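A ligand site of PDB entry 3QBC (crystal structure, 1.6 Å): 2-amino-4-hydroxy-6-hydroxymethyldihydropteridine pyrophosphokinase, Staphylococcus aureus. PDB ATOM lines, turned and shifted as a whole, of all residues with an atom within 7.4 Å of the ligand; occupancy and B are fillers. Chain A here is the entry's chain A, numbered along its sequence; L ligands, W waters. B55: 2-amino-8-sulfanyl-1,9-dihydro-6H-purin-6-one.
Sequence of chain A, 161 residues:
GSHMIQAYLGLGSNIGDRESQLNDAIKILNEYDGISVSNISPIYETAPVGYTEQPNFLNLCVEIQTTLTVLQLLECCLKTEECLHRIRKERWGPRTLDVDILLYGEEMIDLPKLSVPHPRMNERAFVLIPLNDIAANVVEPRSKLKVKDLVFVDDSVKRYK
A nitrogen (N3) of the ligand sits at hydrogen-bond distance from the backbone carbonyl oxygen (O) of Ala 47. The backbone NH of Val 49 lies within hydrogen-bond range of a nitrogen (N2) of the ligand (2.9 Å). A nitrogen (N5) of the ligand lies within hydrogen-bond range of the backbone carbonyl oxygen (O) of Val 49. The side-chain amide nitrogen (ND2) of Asn 59 sits at hydrogen-bond distance from an oxygen (O1) of the ligand. N3 of the ligand is in hydrogen-bond range of OG1 of Thr 46, 3.0 Å away.
Water W1 lies within hydrogen-bond range of NE2 of Gln 54, N of Tyr 51, O of Val 49 and S1 of the ligand.
The backbone carbonyl oxygen (O) of Ser 156 lies within hydrogen-bond range of the backbone NH (N) of Ala 47 (3.0 Å). The side-chain amide oxygen of Asn 59 is in hydrogen-bond range of the side-chain hydroxyl of Thr 46 (2.7 Å). The backbone carbonyl oxygen of Leu 11 sits at hydrogen-bond distance from the side-chain amide nitrogen of Asn 59 (3.0 Å). N of Thr 46 sits at hydrogen-bond distance from O of Phe 57, at 2.8 Å. O of Gly 12 is in hydrogen-bond range of N of Asp 98, 2.9 Å away.
Gly 12 touches the ligand (CA to O1, 3.97 Å). Pro 48 touches the ligand. Phe 57 touches the ligand. Phe 126 touches the ligand. Hydrophobic or aromatic side chains that line the ligand: Val 49, Phe 57 and Phe 126. Eight residues have an atom within 4 Å of the ligand: Gly 12, Thr 46, Ala 47, Pro 48, Val 49, Phe 57, Asn 59 and Phe 126.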
ATOM      1  N   GLY A  10       3.318 -23.268   9.534  1.00  0.00           N
ATOM      2  CA  GLY A  10       2.807 -23.578   8.160  1.00  0.00           C
ATOM      3  C   GLY A  10       3.387 -22.473   7.232  1.00  0.00           C
ATOM      4  O   GLY A  10       3.279 -21.281   7.583  1.00  0.00           O
ATOM      5  N   LEU A  11       3.949 -22.840   6.070  1.00  0.00           N
ATOM      6  CA  LEU A  11       4.509 -21.855   5.165  1.00  0.00           C
ATOM      7  C   LEU A  11       3.932 -22.070   3.769  1.00  0.00           C
ATOM      8  O   LEU A  11       3.581 -23.185   3.405  1.00  0.00           O
ATOM      9  CB  LEU A  11       6.032 -21.983   5.003  1.00  0.00           C
ATOM     10  CG  LEU A  11       6.853 -21.527   6.220  1.00  0.00           C
ATOM     11  CD1 LEU A  11       6.841 -22.443   7.457  1.00  0.00           C
ATOM     12  CD2 LEU A  11       8.250 -21.367   5.748  1.00  0.00           C
ATOM     13  N   GLY A  12       3.774 -20.954   3.066  1.00  0.00           N
ATOM     14  CA  GLY A  12       3.154 -21.041   1.723  1.00  0.00           C
ATOM     15  C   GLY A  12       3.603 -19.932   0.833  1.00  0.00           C
ATOM     16  O   GLY A  12       3.942 -18.841   1.310  1.00  0.00           O
ATOM     17  N   SER A  13       3.670 -20.208  -0.489  1.00  0.00           N
ATOM     18  CA  SER A  13       3.991 -19.118  -1.461  1.00  0.00           C
ATOM     19  C   SER A  13       3.398 -19.500  -2.814  1.00  0.00           C
ATOM     20  O   SER A  13       3.474 -20.651  -3.196  1.00  0.00           O
ATOM     21  CB  SER A  13       5.508 -19.003  -1.623  1.00  0.00           C
ATOM     22  OG  SER A  13       5.825 -18.091  -2.689  1.00  0.00           O
ATOM     23  N   ASN A  14       2.781 -18.503  -3.500  1.00  0.00           N
ATOM     24  CA  ASN A  14       2.218 -18.770  -4.834  1.00  0.00           C
ATOM     25  C   ASN A  14       2.731 -17.876  -5.960  1.00  0.00           C
ATOM     26  O   ASN A  14       2.275 -18.009  -7.100  1.00  0.00           O
ATOM     27  CB  ASN A  14       0.665 -18.860  -4.826  1.00  0.00           C
ATOM     28  CG  ASN A  14      -0.025 -17.522  -4.741  1.00  0.00           C
ATOM     29  OD1 ASN A  14       0.493 -16.558  -4.162  1.00  0.00           O
ATOM     30  ND2 ASN A  14      -1.261 -17.453  -5.266  1.00  0.00           N
ATOM     31  N   GLU A  45       2.144 -29.099  -3.684  1.00  0.00           N
ATOM     32  CA  GLU A  45       1.486 -28.100  -4.547  1.00  0.00           C
ATOM     33  C   GLU A  45       0.048 -28.177  -4.295  1.00  0.00           C
ATOM     34  O   GLU A  45      -0.550 -29.250  -4.349  1.00  0.00           O
ATOM     35  CB  GLU A  45       1.876 -28.299  -6.024  1.00  0.00           C
ATOM     36  CG  GLU A  45       1.178 -27.189  -6.882  1.00  0.00           C
ATOM     37  CD  GLU A  45       1.795 -27.071  -8.249  1.00  0.00           C
ATOM     38  OE1 GLU A  45       1.618 -28.092  -8.925  1.00  0.00           O
ATOM     39  OE2 GLU A  45       2.398 -26.020  -8.658  1.00  0.00           O
ATOM     40  N   THR A  46      -0.565 -27.003  -4.100  1.00  0.00           N
ATOM     41  CA  THR A  46      -1.950 -26.979  -3.623  1.00  0.00           C
ATOM     42  C   THR A  46      -2.806 -25.928  -4.315  1.00  0.00           C
ATOM     43  O   THR A  46      -2.353 -24.826  -4.622  1.00  0.00           O
ATOM     44  CB  THR A  46      -2.001 -26.681  -2.082  1.00  0.00           C
ATOM     45  OG1 THR A  46      -1.408 -25.395  -1.836  1.00  0.00           O
ATOM     46  CG2 THR A  46      -1.135 -27.715  -1.340  1.00  0.00           C
ATOM     47  N   ALA A  47      -3.981 -26.323  -4.666  1.00  0.00           N
ATOM     48  CA  ALA A  47      -4.885 -25.369  -5.330  1.00  0.00           C
ATOM     49  C   ALA A  47      -5.210 -24.258  -4.335  1.00  0.00           C
ATOM     50  O   ALA A  47      -5.354 -24.465  -3.118  1.00  0.00           O
ATOM     51  CB  ALA A  47      -6.160 -26.085  -5.781  1.00  0.00           C
ATOM     52  N   PRO A  48      -5.393 -23.038  -4.868  1.00  0.00           N
ATOM     53  CA  PRO A  48      -5.570 -21.885  -4.002  1.00  0.00           C
ATOM     54  C   PRO A  48      -6.874 -21.933  -3.259  1.00  0.00           C
ATOM     55  O   PRO A  48      -7.929 -22.303  -3.829  1.00  0.00           O
ATOM     56  CB  PRO A  48      -5.528 -20.677  -4.991  1.00  0.00           C
ATOM     57  CG  PRO A  48      -5.732 -21.273  -6.325  1.00  0.00           C
ATOM     58  CD  PRO A  48      -5.226 -22.704  -6.295  1.00  0.00           C
ATOM     59  N   VAL A  49      -6.834 -21.528  -1.985  1.00  0.00           N
ATOM     60  CA  VAL A  49      -8.053 -21.533  -1.156  1.00  0.00           C
ATOM     61  C   VAL A  49      -8.353 -20.028  -0.929  1.00  0.00           C
ATOM     62  O   VAL A  49      -7.451 -19.231  -0.647  1.00  0.00           O
ATOM     63  CB  VAL A  49      -7.865 -22.195   0.234  1.00  0.00           C
ATOM     64  CG1 VAL A  49      -9.127 -21.996   1.063  1.00  0.00           C
ATOM     65  CG2 VAL A  49      -7.472 -23.651   0.090  1.00  0.00           C
ATOM     66  N   GLY A  50      -9.614 -19.624  -1.055  1.00  0.00           N
ATOM     67  CA  GLY A  50      -9.992 -18.198  -0.863  1.00  0.00           C
ATOM     68  C   GLY A  50     -10.313 -17.687  -2.241  1.00  0.00           C
ATOM     69  O   GLY A  50     -11.251 -18.165  -2.875  1.00  0.00           O
ATOM     70  N   TYR A  51      -9.419 -16.911  -2.829  1.00  0.00           N
ATOM     71  CA  TYR A  51      -9.677 -16.460  -4.221  1.00  0.00           C
ATOM     72  C   TYR A  51      -9.240 -17.620  -5.137  1.00  0.00           C
ATOM     73  O   TYR A  51      -8.132 -18.117  -5.004  1.00  0.00           O
ATOM     74  CB  TYR A  51      -8.798 -15.291  -4.585  1.00  0.00           C
ATOM     75  CG  TYR A  51      -8.941 -14.029  -3.819  1.00  0.00           C
ATOM     76  CD1 TYR A  51     -10.181 -13.517  -3.516  1.00  0.00           C
ATOM     77  CD2 TYR A  51      -7.773 -13.321  -3.443  1.00  0.00           C
ATOM     78  CE1 TYR A  51     -10.296 -12.308  -2.834  1.00  0.00           C
ATOM     79  CE2 TYR A  51      -7.880 -12.095  -2.772  1.00  0.00           C
ATOM     80  CZ  TYR A  51      -9.157 -11.623  -2.469  1.00  0.00           C
ATOM     81  OH  TYR A  51      -9.326 -10.441  -1.833  1.00  0.00           O
ATOM     82  N   GLN A  54      -5.946 -17.372  -8.894  1.00  0.00           N
ATOM     83  CA  GLN A  54      -4.577 -17.000  -8.586  1.00  0.00           C
ATOM     84  C   GLN A  54      -3.731 -18.285  -8.649  1.00  0.00           C
ATOM     85  O   GLN A  54      -4.261 -19.366  -8.742  1.00  0.00           O
ATOM     86  CB  GLN A  54      -4.509 -16.399  -7.166  1.00  0.00           C
ATOM     87  CG  GLN A  54      -4.905 -17.418  -6.041  1.00  0.00           C
ATOM     88  CD  GLN A  54      -4.767 -16.825  -4.685  1.00  0.00           C
ATOM     89  OE1 GLN A  54      -3.755 -16.142  -4.401  1.00  0.00           O
ATOM     90  NE2 GLN A  54      -5.706 -17.139  -3.826  1.00  0.00           N
ATOM     91  N   PRO A  55      -2.424 -18.153  -8.605  1.00  0.00           N
ATOM     92  CA  PRO A  55      -1.622 -19.373  -8.865  1.00  0.00           C
ATOM     93  C   PRO A  55      -1.674 -20.402  -7.783  1.00  0.00           C
ATOM     94  O   PRO A  55      -1.910 -20.069  -6.624  1.00  0.00           O
ATOM     95  CB  PRO A  55      -0.189 -18.840  -8.974  1.00  0.00           C
ATOM     96  CG  PRO A  55      -0.399 -17.399  -9.530  1.00  0.00           C
ATOM     97  CD  PRO A  55      -1.600 -16.931  -8.654  1.00  0.00           C
ATOM     98  N   ASN A  56      -1.298 -21.655  -8.135  1.00  0.00           N
ATOM     99  CA  ASN A  56      -1.235 -22.630  -7.121  1.00  0.00           C
ATOM    100  C   ASN A  56      -0.145 -22.303  -6.100  1.00  0.00           C
ATOM    101  O   ASN A  56       0.885 -21.728  -6.450  1.00  0.00           O
ATOM    102  CB  ASN A  56      -0.819 -23.930  -7.780  1.00  0.00           C
ATOM    103  CG  ASN A  56      -1.709 -24.292  -8.909  1.00  0.00           C
ATOM    104  OD1 ASN A  56      -2.916 -24.133  -8.784  1.00  0.00           O
ATOM    105  ND2 ASN A  56      -1.111 -24.896  -9.999  1.00  0.00           N
ATOM    106  N   PHE A  57      -0.383 -22.692  -4.859  1.00  0.00           N
ATOM    107  CA  PHE A  57       0.637 -22.571  -3.833  1.00  0.00           C
ATOM    108  C   PHE A  57       1.594 -23.733  -3.742  1.00  0.00           C
ATOM    109  O   PHE A  57       1.223 -24.870  -4.128  1.00  0.00           O
ATOM    110  CB  PHE A  57      -0.019 -22.404  -2.412  1.00  0.00           C
ATOM    111  CG  PHE A  57      -0.677 -21.067  -2.201  1.00  0.00           C
ATOM    112  CD1 PHE A  57      -0.048 -20.153  -1.456  1.00  0.00           C
ATOM    113  CD2 PHE A  57      -1.916 -20.766  -2.854  1.00  0.00           C
ATOM    114  CE1 PHE A  57      -0.641 -18.875  -1.284  1.00  0.00           C
ATOM    115  CE2 PHE A  57      -2.507 -19.512  -2.714  1.00  0.00           C
ATOM    116  CZ  PHE A  57      -1.864 -18.570  -1.951  1.00  0.00           C
ATOM    117  N   LEU A  58       2.820 -23.460  -3.300  1.00  0.00           N
ATOM    118  CA  LEU A  58       3.555 -24.548  -2.615  1.00  0.00           C
ATOM    119  C   LEU A  58       3.412 -24.299  -1.094  1.00  0.00           C
ATOM    120  O   LEU A  58       3.510 -23.166  -0.614  1.00  0.00           O
ATOM    121  CB  LEU A  58       5.024 -24.466  -2.966  1.00  0.00           C
ATOM    122  CG  LEU A  58       5.455 -24.677  -4.431  1.00  0.00           C
ATOM    123  CD1 LEU A  58       7.021 -24.737  -4.651  1.00  0.00           C
ATOM    124  CD2 LEU A  58       4.759 -25.896  -4.941  1.00  0.00           C
ATOM    125  N   ASN A  59       3.204 -25.381  -0.355  1.00  0.00           N
ATOM    126  CA  ASN A  59       3.047 -25.334   1.098  1.00  0.00           C
ATOM    127  C   ASN A  59       3.921 -26.403   1.743  1.00  0.00           C
ATOM    128  O   ASN A  59       4.072 -27.474   1.187  1.00  0.00           O
ATOM    129  CB  ASN A  59       1.611 -25.671   1.461  1.00  0.00           C
ATOM    130  CG  ASN A  59       0.691 -24.481   1.292  1.00  0.00           C
ATOM    131  OD1 ASN A  59      -0.196 -24.474   0.417  1.00  0.00           O
ATOM    132  ND2 ASN A  59       0.898 -23.450   2.110  1.00  0.00           N
ATOM    133  N   LEU A  60       4.422 -26.057   2.919  1.00  0.00           N
ATOM    134  CA  LEU A  60       5.033 -27.107   3.741  1.00  0.00           C
ATOM    135  C   LEU A  60       4.756 -26.773   5.192  1.00  0.00           C
ATOM    136  O   LEU A  60       4.205 -25.717   5.535  1.00  0.00           O
ATOM    137  CB  LEU A  60       6.532 -27.245   3.450  1.00  0.00           C
ATOM    138  CG  LEU A  60       7.433 -26.020   3.576  1.00  0.00           C
ATOM    139  CD1 LEU A  60       7.760 -25.676   5.036  1.00  0.00           C
ATOM    140  CD2 LEU A  60       8.791 -26.280   2.919  1.00  0.00           C
ATOM    141  N   ASP A  98       3.758 -16.668   3.170  1.00  0.00           N
ATOM    142  CA  ASP A  98       3.055 -16.598   4.447  1.00  0.00           C
ATOM    143  C   ASP A  98       3.612 -17.594   5.412  1.00  0.00           C
ATOM    144  O   ASP A  98       3.883 -18.716   5.010  1.00  0.00           O
ATOM    145  CB  ASP A  98       1.608 -16.893   4.239  1.00  0.00           C
ATOM    146  CG  ASP A  98       0.973 -15.888   3.288  1.00  0.00           C
ATOM    147  OD1 ASP A  98       1.198 -14.683   3.493  1.00  0.00           O
ATOM    148  OD2 ASP A  98       0.337 -16.345   2.305  1.00  0.00           O
ATOM    149  N   ASP A 100       2.608 -19.087   9.248  1.00  0.00           N
ATOM    150  CA  ASP A 100       1.633 -19.088  10.300  1.00  0.00           C
ATOM    151  C   ASP A 100       2.041 -20.034  11.427  1.00  0.00           C
ATOM    152  O   ASP A 100       2.693 -21.047  11.170  1.00  0.00           O
ATOM    153  CB  ASP A 100       0.254 -19.615   9.807  1.00  0.00           C
ATOM    154  CG  ASP A 100      -0.323 -18.751   8.788  1.00  0.00           C
ATOM    155  OD1 ASP A 100      -0.205 -17.537   9.003  1.00  0.00           O
ATOM    156  OD2 ASP A 100      -0.878 -19.292   7.819  1.00  0.00           O
ATOM    157  N   ARG A 124      -8.151 -26.917   6.419  1.00  0.00           N
ATOM    158  CA  ARG A 124      -7.202 -26.747   5.320  1.00  0.00           C
ATOM    159  C   ARG A 124      -6.271 -27.907   5.064  1.00  0.00           C
ATOM    160  O   ARG A 124      -5.277 -28.119   5.784  1.00  0.00           O
ATOM    161  CB  ARG A 124      -6.394 -25.496   5.544  1.00  0.00           C
ATOM    162  CG  ARG A 124      -7.239 -24.273   5.333  1.00  0.00           C
ATOM    163  CD  ARG A 124      -6.743 -23.165   6.127  1.00  0.00           C
ATOM    164  NE  ARG A 124      -7.804 -22.155   6.114  1.00  0.00           N
ATOM    165  CZ  ARG A 124      -7.761 -21.044   6.814  1.00  0.00           C
ATOM    166  NH1 ARG A 124      -6.716 -20.819   7.597  1.00  0.00           N
ATOM    167  NH2 ARG A 124      -8.784 -20.168   6.726  1.00  0.00           N
ATOM    168  N   ALA A 125      -6.544 -28.629   3.985  1.00  0.00           N
ATOM    169  CA  ALA A 125      -5.716 -29.752   3.622  1.00  0.00           C
ATOM    170  C   ALA A 125      -4.291 -29.299   3.336  1.00  0.00           C
ATOM    171  O   ALA A 125      -3.360 -30.085   3.539  1.00  0.00           O
ATOM    172  CB  ALA A 125      -6.257 -30.494   2.355  1.00  0.00           C
ATOM    173  N   PHE A 126      -4.123 -28.055   2.859  1.00  0.00           N
ATOM    174  CA  PHE A 126      -2.759 -27.617   2.531  1.00  0.00           C
ATOM    175  C   PHE A 126      -1.936 -27.450   3.782  1.00  0.00           C
ATOM    176  O   PHE A 126      -0.712 -27.291   3.654  1.00  0.00           O
ATOM    177  CB  PHE A 126      -2.845 -26.353   1.642  1.00  0.00           C
ATOM    178  CG  PHE A 126      -3.317 -25.087   2.358  1.00  0.00           C
ATOM    179  CD1 PHE A 126      -2.385 -24.361   3.146  1.00  0.00           C
ATOM    180  CD2 PHE A 126      -4.612 -24.572   2.163  1.00  0.00           C
ATOM    181  CE1 PHE A 126      -2.777 -23.184   3.808  1.00  0.00           C
ATOM    182  CE2 PHE A 126      -5.000 -23.314   2.731  1.00  0.00           C
ATOM    183  CZ  PHE A 126      -4.056 -22.641   3.607  1.00  0.00           C
ATOM    184  N   VAL A 127      -2.592 -27.386   4.944  1.00  0.00           N
ATOM    185  CA  VAL A 127      -1.930 -27.416   6.250  1.00  0.00           C
ATOM    186  C   VAL A 127      -1.817 -28.859   6.703  1.00  0.00           C
ATOM    187  O   VAL A 127      -0.734 -29.351   7.050  1.00  0.00           O
ATOM    188  CB  VAL A 127      -2.642 -26.542   7.288  1.00  0.00           C
ATOM    189  CG1 VAL A 127      -2.036 -26.790   8.671  1.00  0.00           C
ATOM    190  CG2 VAL A 127      -2.659 -25.044   6.901  1.00  0.00           C
ATOM    191  N   SER A 156      -6.800 -31.834  -4.305  1.00  0.00           N
ATOM    192  CA  SER A 156      -6.219 -30.580  -4.724  1.00  0.00           C
ATOM    193  C   SER A 156      -4.836 -30.353  -4.067  1.00  0.00           C
ATOM    194  O   SER A 156      -4.235 -29.320  -4.304  1.00  0.00           O
ATOM    195  CB  SER A 156      -7.119 -29.391  -4.412  1.00  0.00           C
ATOM    196  OG  SER A 156      -7.089 -29.038  -3.040  1.00  0.00           O
ATOM    197  N   VAL A 157      -4.388 -31.317  -3.231  1.00  0.00           N
ATOM    198  CA  VAL A 157      -3.084 -31.192  -2.593  1.00  0.00           C
ATOM    199  C   VAL A 157      -2.243 -32.389  -3.050  1.00  0.00           C
ATOM    200  O   VAL A 157      -2.671 -33.532  -2.871  1.00  0.00           O
ATOM    201  CB  VAL A 157      -3.260 -31.248  -1.055  1.00  0.00           C
ATOM    202  CG1 VAL A 157      -1.918 -31.402  -0.316  1.00  0.00           C
ATOM    203  CG2 VAL A 157      -4.039 -30.058  -0.589  1.00  0.00           C
HETATM  204  O1  B55 L   1      -0.815 -21.160   1.734  1.00  0.00           O
HETATM  205  C5  B55 L   1      -1.877 -21.258   1.118  1.00  0.00           C
HETATM  206  C2  B55 L   1      -2.892 -20.215   0.998  1.00  0.00           C
HETATM  207  N1  B55 L   1      -2.936 -18.939   1.539  1.00  0.00           N
HETATM  208  N4  B55 L   1      -2.292 -22.358   0.371  1.00  0.00           N
HETATM  209  C4  B55 L   1      -3.468 -22.492  -0.349  1.00  0.00           C
HETATM  210  N3  B55 L   1      -3.672 -23.663  -1.007  1.00  0.00           N
HETATM  211  N2  B55 L   1      -4.357 -21.552  -0.475  1.00  0.00           N
HETATM  212  C3  B55 L   1      -3.977 -20.468   0.256  1.00  0.00           C
HETATM  213  N5  B55 L   1      -4.756 -19.306   0.326  1.00  0.00           N
HETATM  214  C1  B55 L   1      -4.059 -18.440   1.085  1.00  0.00           C
HETATM  215  S1  B55 L   1      -4.693 -16.827   1.360  1.00  0.00           S
HETATM  216  O   HOH W   1      -6.718 -16.208  -1.339  1.00  0.00           O
